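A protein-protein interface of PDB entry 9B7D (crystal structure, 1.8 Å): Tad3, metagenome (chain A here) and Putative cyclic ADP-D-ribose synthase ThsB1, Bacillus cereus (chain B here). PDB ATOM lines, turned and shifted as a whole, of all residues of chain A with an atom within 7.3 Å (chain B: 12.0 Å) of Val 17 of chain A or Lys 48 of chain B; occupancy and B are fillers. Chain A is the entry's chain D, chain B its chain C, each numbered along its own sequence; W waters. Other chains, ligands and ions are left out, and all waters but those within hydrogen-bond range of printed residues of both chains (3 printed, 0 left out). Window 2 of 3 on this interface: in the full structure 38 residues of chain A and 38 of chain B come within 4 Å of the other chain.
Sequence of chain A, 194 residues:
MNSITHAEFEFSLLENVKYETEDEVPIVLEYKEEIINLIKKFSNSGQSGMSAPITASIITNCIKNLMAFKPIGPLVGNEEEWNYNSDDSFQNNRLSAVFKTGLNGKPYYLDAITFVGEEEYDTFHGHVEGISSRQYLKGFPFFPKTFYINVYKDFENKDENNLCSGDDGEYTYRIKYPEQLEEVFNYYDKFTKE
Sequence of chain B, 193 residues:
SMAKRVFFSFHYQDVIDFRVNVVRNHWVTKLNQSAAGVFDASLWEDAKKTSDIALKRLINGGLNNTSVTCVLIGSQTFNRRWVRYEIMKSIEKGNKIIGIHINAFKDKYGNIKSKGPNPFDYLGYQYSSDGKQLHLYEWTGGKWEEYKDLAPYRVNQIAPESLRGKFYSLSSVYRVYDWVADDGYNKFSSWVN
OD1 of Asp 46 of chain B sits close to N of Lys 48 of chain B (3.1 Å). OG1 of Thr 50 of chain B lies within hydrogen-bond range of O of Ala 47 of chain B, at 3.3 Å. The backbone carbonyl oxygen of Leu 14 of chain A is in hydrogen-bond range of the side-chain hydroxyl of Tyr 19 of chain A.
Water W1 bridges O of Val 25 of chain A (2.6 Å) and OD2 of Asp 52 of chain B (3.1 Å). Water W3 lies within hydrogen-bond range of O of Lys 48 of chain B (2.6 Å) and O of Glu 24 of chain A (2.8 Å). Water W2 lies within hydrogen-bond range of O of Ala 47 of chain B, O of Thr 50 of chain B, N of Val 28 of chain A and N of Ile 27 of chain A.
O of Thr 50 of chain B sits at hydrogen-bond distance from N of Ile 27 of chain A (3.0 Å).
Among the printed residues, pairs that only touch across the chains: Tyr 19 of chain A with Lys 48 of chain B, Pro 26 of chain A with Ala 47 of chain B, Glu 24 of chain A with Ser 51 of chain B, Ile 27 of chain A with Ser 51 of chain B, Val 25 of chain A with Ser 51 of chain B, Ile 27 of chain A with Asp 52 of chain B, Val 17 of chain A with Lys 48 of chain B, Glu 24 of chain A with Ile 53 of chain B, Pro 26 of chain A with Thr 50 of chain B, Pro 26 of chain A with Lys 48 of chain B, Leu 14 of chain A with Lys 48 of chain B and Val 28 of chain A with Ala 47 of chain B.
Hydrophobic or aromatic side chains of chain B that line the printed part of chain A: Ala 47 and Ile 53. Along chain B the printed residues that touch a printed residue of chain A span positions 47 to 53. Hydrophobic or aromatic side chains of chain A that line the printed part of chain B: Leu 14, Val 17, Tyr 19, Pro 26, Ile 27 and Val 28.
Of chain B, only Lys 48 comes within 4 Å of Leu 14 of chain A. No residue of chain B comes within 4 Å of Asn 16 of chain A. Of chain B, only Lys 48 comes within 4 Å of Val 17 of chain A. No residue of chain B comes within 4 Å of Lys 18 of chain A. Tyr 19 of chain A touches just one residue of chain B: Lys 48 (3.2 Å). Of the printed residues of chain B, Glu 24 of chain A touches Ser 51 and Ile 53. Of chain B, only Ala 47 (3.2 Å), Lys 48 (3.8 Å) and Thr 50 (3.7 Å) come within 4 Å of Pro 26 of chain A. Lys 48 of chain B touches just these residues of chain A: Leu 14 (3.8 Å), Val 17 (3.6 Å), Tyr 19 (3.2 Å) and Pro 26 (3.8 Å). Of the printed residues of chain A, Ser 51 of chain B touches Glu 24, Val 25 and Ile 27. The nearest printed residue of chain A that does not touch Asp 52 of chain B is Val 25 of chain A (4.1 Å).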
ATOM      1  N   PHE A  11       1.812 -26.708  22.014  1.00  0.00           N
ATOM      2  CA  PHE A  11       2.796 -25.706  21.615  1.00  0.00           C
ATOM      3  C   PHE A  11       2.612 -25.296  20.159  1.00  0.00           C
ATOM      4  O   PHE A  11       2.810 -24.122  19.819  1.00  0.00           O
ATOM      5  CB  PHE A  11       4.214 -26.219  21.854  1.00  0.00           C
ATOM      6  CG  PHE A  11       4.658 -26.110  23.288  1.00  0.00           C
ATOM      7  CD1 PHE A  11       4.983 -24.878  23.838  1.00  0.00           C
ATOM      8  CD2 PHE A  11       4.734 -27.239  24.089  1.00  0.00           C
ATOM      9  CE1 PHE A  11       5.383 -24.772  25.158  1.00  0.00           C
ATOM     10  CE2 PHE A  11       5.130 -27.142  25.412  1.00  0.00           C
ATOM     11  CZ  PHE A  11       5.457 -25.907  25.949  1.00  0.00           C
ATOM     12  N   SER A  12       2.218 -26.235  19.293  1.00  0.00           N
ATOM     13  CA  SER A  12       2.024 -25.901  17.885  1.00  0.00           C
ATOM     14  C   SER A  12       0.921 -24.865  17.700  1.00  0.00           C
ATOM     15  O   SER A  12       0.997 -24.040  16.782  1.00  0.00           O
ATOM     16  CB  SER A  12       1.716 -27.164  17.076  1.00  0.00           C
ATOM     17  OG  SER A  12       0.345 -27.511  17.167  1.00  0.00           O
ATOM     18  N   LEU A  13      -0.100 -24.886  18.560  1.00  0.00           N
ATOM     19  CA  LEU A  13      -1.148 -23.871  18.498  1.00  0.00           C
ATOM     20  C   LEU A  13      -0.593 -22.475  18.757  1.00  0.00           C
ATOM     21  O   LEU A  13      -1.039 -21.498  18.144  1.00  0.00           O
ATOM     22  CB  LEU A  13      -2.247 -24.200  19.505  1.00  0.00           C
ATOM     23  CG  LEU A  13      -3.517 -24.840  18.955  1.00  0.00           C
ATOM     24  CD1 LEU A  13      -3.183 -25.939  17.974  1.00  0.00           C
ATOM     25  CD2 LEU A  13      -4.329 -25.397  20.107  1.00  0.00           C
ATOM     26  N   LEU A  14       0.368 -22.362  19.677  1.00  0.00           N
ATOM     27  CA  LEU A  14       1.005 -21.071  19.930  1.00  0.00           C
ATOM     28  C   LEU A  14       1.952 -20.696  18.798  1.00  0.00           C
ATOM     29  O   LEU A  14       2.081 -19.516  18.449  1.00  0.00           O
ATOM     30  CB  LEU A  14       1.761 -21.117  21.261  1.00  0.00           C
ATOM     31  CG  LEU A  14       0.954 -21.454  22.516  1.00  0.00           C
ATOM     32  CD1 LEU A  14       1.814 -21.221  23.736  1.00  0.00           C
ATOM     33  CD2 LEU A  14      -0.295 -20.608  22.601  1.00  0.00           C
ATOM     34  N   GLU A  15       2.629 -21.689  18.217  1.00  0.00           N
ATOM     35  CA  GLU A  15       3.623 -21.426  17.183  1.00  0.00           C
ATOM     36  C   GLU A  15       2.983 -21.056  15.849  1.00  0.00           C
ATOM     37  O   GLU A  15       3.554 -20.261  15.094  1.00  0.00           O
ATOM     38  CB  GLU A  15       4.536 -22.649  17.014  1.00  0.00           C
ATOM     39  CG  GLU A  15       5.392 -22.958  18.250  1.00  0.00           C
ATOM     40  CD  GLU A  15       5.895 -24.393  18.286  1.00  0.00           C
ATOM     41  OE1 GLU A  15       5.243 -25.280  17.690  1.00  0.00           O
ATOM     42  OE2 GLU A  15       6.942 -24.638  18.925  1.00  0.00           O
ATOM     43  N   ASN A  16       1.807 -21.600  15.547  1.00  0.00           N
ATOM     44  CA  ASN A  16       1.153 -21.377  14.258  1.00  0.00           C
ATOM     45  C   ASN A  16       0.481 -20.010  14.130  1.00  0.00           C
ATOM     46  O   ASN A  16      -0.216 -19.776  13.138  1.00  0.00           O
ATOM     47  CB  ASN A  16       0.122 -22.480  13.987  1.00  0.00           C
ATOM     48  CG  ASN A  16       0.755 -23.852  13.863  1.00  0.00           C
ATOM     49  OD1 ASN A  16       0.065 -24.875  13.873  1.00  0.00           O
ATOM     50  ND2 ASN A  16       2.073 -23.882  13.715  1.00  0.00           N
ATOM     51  N   VAL A  17       0.670 -19.107  15.082  1.00  0.00           N
ATOM     52  CA  VAL A  17       0.048 -17.787  15.044  1.00  0.00           C
ATOM     53  C   VAL A  17       1.071 -16.782  14.536  1.00  0.00           C
ATOM     54  O   VAL A  17       2.255 -16.853  14.890  1.00  0.00           O
ATOM     55  CB  VAL A  17      -0.484 -17.391  16.436  1.00  0.00           C
ATOM     56  CG1 VAL A  17      -0.948 -15.943  16.453  1.00  0.00           C
ATOM     57  CG2 VAL A  17      -1.614 -18.319  16.853  1.00  0.00           C
ATOM     58  N   LYS A  18       0.625 -15.865  13.677  1.00  0.00           N
ATOM     59  CA  LYS A  18       1.470 -14.761  13.230  1.00  0.00           C
ATOM     60  C   LYS A  18       1.375 -13.621  14.237  1.00  0.00           C
ATOM     61  O   LYS A  18       0.294 -13.060  14.445  1.00  0.00           O
ATOM     62  CB  LYS A  18       1.049 -14.275  11.843  1.00  0.00           C
ATOM     63  CG  LYS A  18       1.549 -15.124  10.686  1.00  0.00           C
ATOM     64  CD  LYS A  18       0.403 -15.852  10.002  1.00  0.00           C
ATOM     65  CE  LYS A  18       0.776 -16.248   8.582  1.00  0.00           C
ATOM     66  NZ  LYS A  18      -0.419 -16.332   7.695  1.00  0.00           N
ATOM     67  N   TYR A  19       2.498 -13.280  14.863  1.00  0.00           N
ATOM     68  CA  TYR A  19       2.530 -12.249  15.890  1.00  0.00           C
ATOM     69  C   TYR A  19       3.064 -10.962  15.277  1.00  0.00           C
ATOM     70  O   TYR A  19       4.164 -10.947  14.712  1.00  0.00           O
ATOM     71  CB  TYR A  19       3.379 -12.692  17.082  1.00  0.00           C
ATOM     72  CG  TYR A  19       2.815 -13.921  17.753  1.00  0.00           C
ATOM     73  CD1 TYR A  19       1.677 -13.842  18.544  1.00  0.00           C
ATOM     74  CD2 TYR A  19       3.402 -15.168  17.571  1.00  0.00           C
ATOM     75  CE1 TYR A  19       1.149 -14.963  19.148  1.00  0.00           C
ATOM     76  CE2 TYR A  19       2.878 -16.299  18.169  1.00  0.00           C
ATOM     77  CZ  TYR A  19       1.750 -16.190  18.954  1.00  0.00           C
ATOM     78  OH  TYR A  19       1.222 -17.308  19.553  1.00  0.00           O
ATOM     79  N   GLU A  20       2.276  -9.888  15.380  1.00  0.00           N
ATOM     80  CA  GLU A  20       2.669  -8.618  14.781  1.00  0.00           C
ATOM     81  C   GLU A  20       3.946  -8.078  15.409  1.00  0.00           C
ATOM     82  O   GLU A  20       4.807  -7.532  14.711  1.00  0.00           O
ATOM     83  CB  GLU A  20       1.535  -7.602  14.914  1.00  0.00           C
ATOM     84  CG  GLU A  20       0.502  -7.683  13.799  1.00  0.00           C
ATOM     85  CD  GLU A  20       1.081  -8.247  12.514  1.00  0.00           C
ATOM     86  OE1 GLU A  20       0.600  -9.308  12.058  1.00  0.00           O
ATOM     87  OE2 GLU A  20       2.017  -7.630  11.961  1.00  0.00           O
ATOM     88  N   GLU A  24       4.154  -9.781  21.680  1.00  0.00           N
ATOM     89  CA  GLU A  24       2.947 -10.599  21.694  1.00  0.00           C
ATOM     90  C   GLU A  24       3.224 -12.099  21.746  1.00  0.00           C
ATOM     91  O   GLU A  24       2.290 -12.876  21.975  1.00  0.00           O
ATOM     92  CB  GLU A  24       2.089 -10.288  20.461  1.00  0.00           C
ATOM     93  CG  GLU A  24       1.550  -8.866  20.431  1.00  0.00           C
ATOM     94  CD  GLU A  24       0.561  -8.636  19.305  1.00  0.00           C
ATOM     95  OE1 GLU A  24      -0.642  -8.919  19.498  1.00  0.00           O
ATOM     96  OE2 GLU A  24       0.989  -8.174  18.225  1.00  0.00           O
ATOM     97  N   VAL A  25       4.464 -12.518  21.543  1.00  0.00           N
ATOM     98  CA  VAL A  25       4.795 -13.950  21.544  1.00  0.00           C
ATOM     99  C   VAL A  25       4.571 -14.522  22.941  1.00  0.00           C
ATOM    100  O   VAL A  25       5.089 -13.966  23.923  1.00  0.00           O
ATOM    101  CB  VAL A  25       6.242 -14.154  21.089  1.00  0.00           C
ATOM    102  CG1 VAL A  25       6.642 -15.623  21.201  1.00  0.00           C
ATOM    103  CG2 VAL A  25       6.427 -13.643  19.656  1.00  0.00           C
ATOM    104  N   PRO A  26       3.815 -15.612  23.085  1.00  0.00           N
ATOM    105  CA  PRO A  26       3.585 -16.185  24.419  1.00  0.00           C
ATOM    106  C   PRO A  26       4.887 -16.547  25.125  1.00  0.00           C
ATOM    107  O   PRO A  26       5.810 -17.104  24.527  1.00  0.00           O
ATOM    108  CB  PRO A  26       2.739 -17.429  24.123  1.00  0.00           C
ATOM    109  CG  PRO A  26       2.013 -17.072  22.859  1.00  0.00           C
ATOM    110  CD  PRO A  26       3.014 -16.292  22.052  1.00  0.00           C
ATOM    111  N   ILE A  27       4.941 -16.224  26.420  1.00  0.00           N
ATOM    112  CA  ILE A  27       6.166 -16.401  27.197  1.00  0.00           C
ATOM    113  C   ILE A  27       6.579 -17.870  27.255  1.00  0.00           C
ATOM    114  O   ILE A  27       7.775 -18.183  27.229  1.00  0.00           O
ATOM    115  CB  ILE A  27       5.991 -15.797  28.605  1.00  0.00           C
ATOM    116  CG1 ILE A  27       6.170 -14.278  28.549  1.00  0.00           C
ATOM    117  CG2 ILE A  27       6.976 -16.412  29.604  1.00  0.00           C
ATOM    118  CD1 ILE A  27       5.319 -13.518  29.556  1.00  0.00           C
ATOM    119  N   VAL A  28       5.611 -18.797  27.318  1.00  0.00           N
ATOM    120  CA  VAL A  28       5.964 -20.207  27.515  1.00  0.00           C
ATOM    121  C   VAL A  28       6.786 -20.777  26.370  1.00  0.00           C
ATOM    122  O   VAL A  28       7.491 -21.770  26.567  1.00  0.00           O
ATOM    123  CB  VAL A  28       4.731 -21.124  27.718  1.00  0.00           C
ATOM    124  CG1 VAL A  28       4.250 -21.095  29.147  1.00  0.00           C
ATOM    125  CG2 VAL A  28       3.621 -20.805  26.726  1.00  0.00           C
ATOM    126  N   PHE B  39       0.122 -12.065  40.664  1.00  0.00           N
ATOM    127  CA  PHE B  39      -0.315 -12.783  39.466  1.00  0.00           C
ATOM    128  C   PHE B  39      -0.526 -14.275  39.703  1.00  0.00           C
ATOM    129  O   PHE B  39       0.284 -14.950  40.347  1.00  0.00           O
ATOM    130  CB  PHE B  39       0.715 -12.591  38.350  1.00  0.00           C
ATOM    131  CG  PHE B  39       0.265 -13.106  37.014  1.00  0.00           C
ATOM    132  CD1 PHE B  39      -0.737 -12.464  36.306  1.00  0.00           C
ATOM    133  CD2 PHE B  39       0.833 -14.253  36.477  1.00  0.00           C
ATOM    134  CE1 PHE B  39      -1.151 -12.943  35.074  1.00  0.00           C
ATOM    135  CE2 PHE B  39       0.426 -14.737  35.248  1.00  0.00           C
ATOM    136  CZ  PHE B  39      -0.570 -14.083  34.546  1.00  0.00           C
ATOM    137  N   ALA B  41      -1.582 -17.327  37.074  1.00  0.00           N
ATOM    138  CA  ALA B  41      -1.908 -17.675  35.696  1.00  0.00           C
ATOM    139  C   ALA B  41      -3.060 -18.670  35.583  1.00  0.00           C
ATOM    140  O   ALA B  41      -3.557 -18.886  34.473  1.00  0.00           O
ATOM    141  CB  ALA B  41      -0.675 -18.241  34.990  1.00  0.00           C
ATOM    142  N   SER B  42      -3.493 -19.277  36.689  1.00  0.00           N
ATOM    143  CA  SER B  42      -4.588 -20.240  36.631  1.00  0.00           C
ATOM    144  C   SER B  42      -5.964 -19.580  36.621  1.00  0.00           C
ATOM    145  O   SER B  42      -6.937 -20.219  36.204  1.00  0.00           O
ATOM    146  CB  SER B  42      -4.496 -21.213  37.809  1.00  0.00           C
ATOM    147  OG  SER B  42      -4.837 -20.573  39.026  1.00  0.00           O
ATOM    148  N   LEU B  43      -6.070 -18.324  37.066  1.00  0.00           N
ATOM    149  CA  LEU B  43      -7.369 -17.657  37.084  1.00  0.00           C
ATOM    150  C   LEU B  43      -7.853 -17.355  35.672  1.00  0.00           C
ATOM    151  O   LEU B  43      -9.011 -17.621  35.327  1.00  0.00           O
ATOM    152  CB  LEU B  43      -7.293 -16.370  37.908  1.00  0.00           C
ATOM    153  CG  LEU B  43      -8.531 -15.470  37.840  1.00  0.00           C
ATOM    154  CD1 LEU B  43      -9.581 -15.901  38.857  1.00  0.00           C
ATOM    155  CD2 LEU B  43      -8.156 -14.007  38.039  1.00  0.00           C
ATOM    156  N   TRP B  44      -6.976 -16.806  34.842  1.00  0.00           N
ATOM    157  CA  TRP B  44      -7.346 -16.363  33.508  1.00  0.00           C
ATOM    158  C   TRP B  44      -7.514 -17.533  32.543  1.00  0.00           C
ATOM    159  O   TRP B  44      -7.314 -17.384  31.339  1.00  0.00           O
ATOM    160  CB  TRP B  44      -6.293 -15.393  32.984  1.00  0.00           C
ATOM    161  CG  TRP B  44      -5.712 -14.534  34.066  1.00  0.00           C
ATOM    162  CD1 TRP B  44      -4.498 -14.687  34.674  1.00  0.00           C
ATOM    163  CD2 TRP B  44      -6.324 -13.390  34.675  1.00  0.00           C
ATOM    164  NE1 TRP B  44      -4.317 -13.707  35.622  1.00  0.00           N
ATOM    165  CE2 TRP B  44      -5.422 -12.898  35.642  1.00  0.00           C
ATOM    166  CE3 TRP B  44      -7.546 -12.733  34.497  1.00  0.00           C
ATOM    167  CZ2 TRP B  44      -5.705 -11.780  36.425  1.00  0.00           C
ATOM    168  CZ3 TRP B  44      -7.824 -11.622  35.276  1.00  0.00           C
ATOM    169  CH2 TRP B  44      -6.907 -11.158  36.227  1.00  0.00           C
ATOM    170  N   ASP B  46      -4.839 -18.661  30.012  1.00  0.00           N
ATOM    171  CA  ASP B  46      -4.633 -18.642  28.565  1.00  0.00           C
ATOM    172  C   ASP B  46      -3.181 -18.292  28.243  1.00  0.00           C
ATOM    173  O   ASP B  46      -2.807 -17.116  28.221  1.00  0.00           O
ATOM    174  CB  ASP B  46      -5.600 -17.650  27.902  1.00  0.00           C
ATOM    175  CG  ASP B  46      -5.647 -17.796  26.389  1.00  0.00           C
ATOM    176  OD1 ASP B  46      -4.833 -18.567  25.834  1.00  0.00           O
ATOM    177  OD2 ASP B  46      -6.506 -17.146  25.753  1.00  0.00           O
ATOM    178  N   ALA B  47      -2.367 -19.322  27.989  1.00  0.00           N
ATOM    179  CA  ALA B  47      -0.961 -19.093  27.677  1.00  0.00           C
ATOM    180  C   ALA B  47      -0.778 -18.289  26.397  1.00  0.00           C
ATOM    181  O   ALA B  47       0.297 -17.716  26.188  1.00  0.00           O
ATOM    182  CB  ALA B  47      -0.218 -20.427  27.570  1.00  0.00           C
ATOM    183  N   LYS B  48      -1.805 -18.229  25.543  1.00  0.00           N
ATOM    184  CA  LYS B  48      -1.744 -17.394  24.346  1.00  0.00           C
ATOM    185  C   LYS B  48      -1.691 -15.909  24.689  1.00  0.00           C
ATOM    186  O   LYS B  48      -1.094 -15.123  23.945  1.00  0.00           O
ATOM    187  CB  LYS B  48      -2.948 -17.688  23.451  1.00  0.00           C
ATOM    188  CG  LYS B  48      -2.973 -16.942  22.129  1.00  0.00           C
ATOM    189  CD  LYS B  48      -1.910 -17.439  21.170  1.00  0.00           C
ATOM    190  CE  LYS B  48      -1.805 -16.512  19.970  1.00  0.00           C
ATOM    191  NZ  LYS B  48      -3.130 -15.976  19.533  1.00  0.00           N
ATOM    192  N   LYS B  49      -2.310 -15.506  25.799  1.00  0.00           N
ATOM    193  CA  LYS B  49      -2.404 -14.095  26.149  1.00  0.00           C
ATOM    194  C   LYS B  49      -1.300 -13.634  27.091  1.00  0.00           C
ATOM    195  O   LYS B  49      -1.050 -12.424  27.184  1.00  0.00           O
ATOM    196  CB  LYS B  49      -3.774 -13.801  26.773  1.00  0.00           C
ATOM    197  CG  LYS B  49      -4.943 -14.312  25.933  1.00  0.00           C
ATOM    198  CD  LYS B  49      -5.986 -13.227  25.707  1.00  0.00           C
ATOM    199  CE  LYS B  49      -7.300 -13.811  25.209  1.00  0.00           C
ATOM    200  NZ  LYS B  49      -7.408 -13.714  23.724  1.00  0.00           N
ATOM    201  N   THR B  50      -0.630 -14.557  27.780  1.00  0.00           N
ATOM    202  CA  THR B  50       0.443 -14.197  28.703  1.00  0.00           C
ATOM    203  C   THR B  50       1.738 -14.071  27.908  1.00  0.00           C
ATOM    204  O   THR B  50       2.552 -14.993  27.805  1.00  0.00           O
ATOM    205  CB  THR B  50       0.561 -15.220  29.818  1.00  0.00           C
ATOM    206  OG1 THR B  50       0.525 -16.538  29.256  1.00  0.00           O
ATOM    207  CG2 THR B  50      -0.587 -15.045  30.792  1.00  0.00           C
ATOM    208  N   SER B  51       1.908 -12.897  27.327  1.00  0.00           N
ATOM    209  CA  SER B  51       3.075 -12.524  26.550  1.00  0.00           C
ATOM    210  C   SER B  51       3.807 -11.395  27.272  1.00  0.00           C
ATOM    211  O   SER B  51       3.478 -11.040  28.406  1.00  0.00           O
ATOM    212  CB  SER B  51       2.652 -12.113  25.145  1.00  0.00           C
ATOM    213  OG  SER B  51       1.927 -10.897  25.205  1.00  0.00           O
ATOM    214  N   ASP B  52       4.793 -10.812  26.593  1.00  0.00           N
ATOM    215  CA  ASP B  52       5.575  -9.751  27.221  1.00  0.00           C
ATOM    216  C   ASP B  52       4.765  -8.468  27.399  1.00  0.00           C
ATOM    217  O   ASP B  52       5.036  -7.702  28.330  1.00  0.00           O
ATOM    218  CB  ASP B  52       6.847  -9.485  26.416  1.00  0.00           C
ATOM    219  CG  ASP B  52       7.935 -10.510  26.692  1.00  0.00           C
ATOM    220  OD1 ASP B  52       7.800 -11.282  27.663  1.00  0.00           O
ATOM    221  OD2 ASP B  52       8.930 -10.548  25.941  1.00  0.00           O
ATOM    222  N   ILE B  53       3.767  -8.210  26.544  1.00  0.00           N
ATOM    223  CA  ILE B  53       2.936  -7.029  26.788  1.00  0.00           C
ATOM    224  C   ILE B  53       2.114  -7.204  28.052  1.00  0.00           C
ATOM    225  O   ILE B  53       1.847  -6.230  28.765  1.00  0.00           O
ATOM    226  CB  ILE B  53       2.021  -6.688  25.593  1.00  0.00           C
ATOM    227  CG1 ILE B  53       1.476  -7.947  24.924  1.00  0.00           C
ATOM    228  CG2 ILE B  53       2.731  -5.774  24.610  1.00  0.00           C
ATOM    229  CD1 ILE B  53       0.614  -7.666  23.712  1.00  0.00           C
ATOM    230  N   ALA B  54       1.692  -8.435  28.356  1.00  0.00           N
ATOM    231  CA  ALA B  54       0.999  -8.676  29.617  1.00  0.00           C
ATOM    232  C   ALA B  54       1.919  -8.424  30.802  1.00  0.00           C
ATOM    233  O   ALA B  54       1.496  -7.870  31.823  1.00  0.00           O
ATOM    234  CB  ALA B  54       0.448 -10.102  29.653  1.00  0.00           C
ATOM    235  N   LEU B  55       3.187  -8.827  30.683  1.00  0.00           N
ATOM    236  CA  LEU B  55       4.176  -8.538  31.713  1.00  0.00           C
ATOM    237  C   LEU B  55       4.358  -7.035  31.890  1.00  0.00           C
ATOM    238  O   LEU B  55       4.414  -6.529  33.018  1.00  0.00           O
ATOM    239  CB  LEU B  55       5.507  -9.191  31.341  1.00  0.00           C
ATOM    240  CG  LEU B  55       6.471  -9.703  32.408  1.00  0.00           C
ATOM    241  CD1 LEU B  55       5.735 -10.124  33.636  1.00  0.00           C
ATOM    242  CD2 LEU B  55       7.277 -10.873  31.860  1.00  0.00           C
ATOM    243  N   ARG B  57       2.240  -4.675  31.231  1.00  0.00           N
ATOM    244  CA  ARG B  57       1.044  -4.088  31.830  1.00  0.00           C
ATOM    245  C   ARG B  57       1.020  -4.276  33.344  1.00  0.00           C
ATOM    246  O   ARG B  57       0.600  -3.376  34.080  1.00  0.00           O
ATOM    247  CB  ARG B  57      -0.206  -4.690  31.189  1.00  0.00           C
ATOM    248  CG  ARG B  57      -0.515  -4.115  29.826  1.00  0.00           C
ATOM    249  CD  ARG B  57      -1.930  -4.450  29.386  1.00  0.00           C
ATOM    250  NE  ARG B  57      -2.028  -4.469  27.932  1.00  0.00           N
ATOM    251  CZ  ARG B  57      -2.443  -5.508  27.221  1.00  0.00           C
ATOM    252  NH1 ARG B  57      -2.816  -6.638  27.802  1.00  0.00           N
ATOM    253  NH2 ARG B  57      -2.477  -5.415  25.895  1.00  0.00           N
HETATM  254  O   HOH W   1       6.785 -12.081  24.251  1.00  0.00           O
HETATM  255  O   HOH W   2       2.751 -17.927  27.697  1.00  0.00           O
HETATM  256  O   HOH W   3      -0.427 -12.930  22.638  1.00  0.00           O
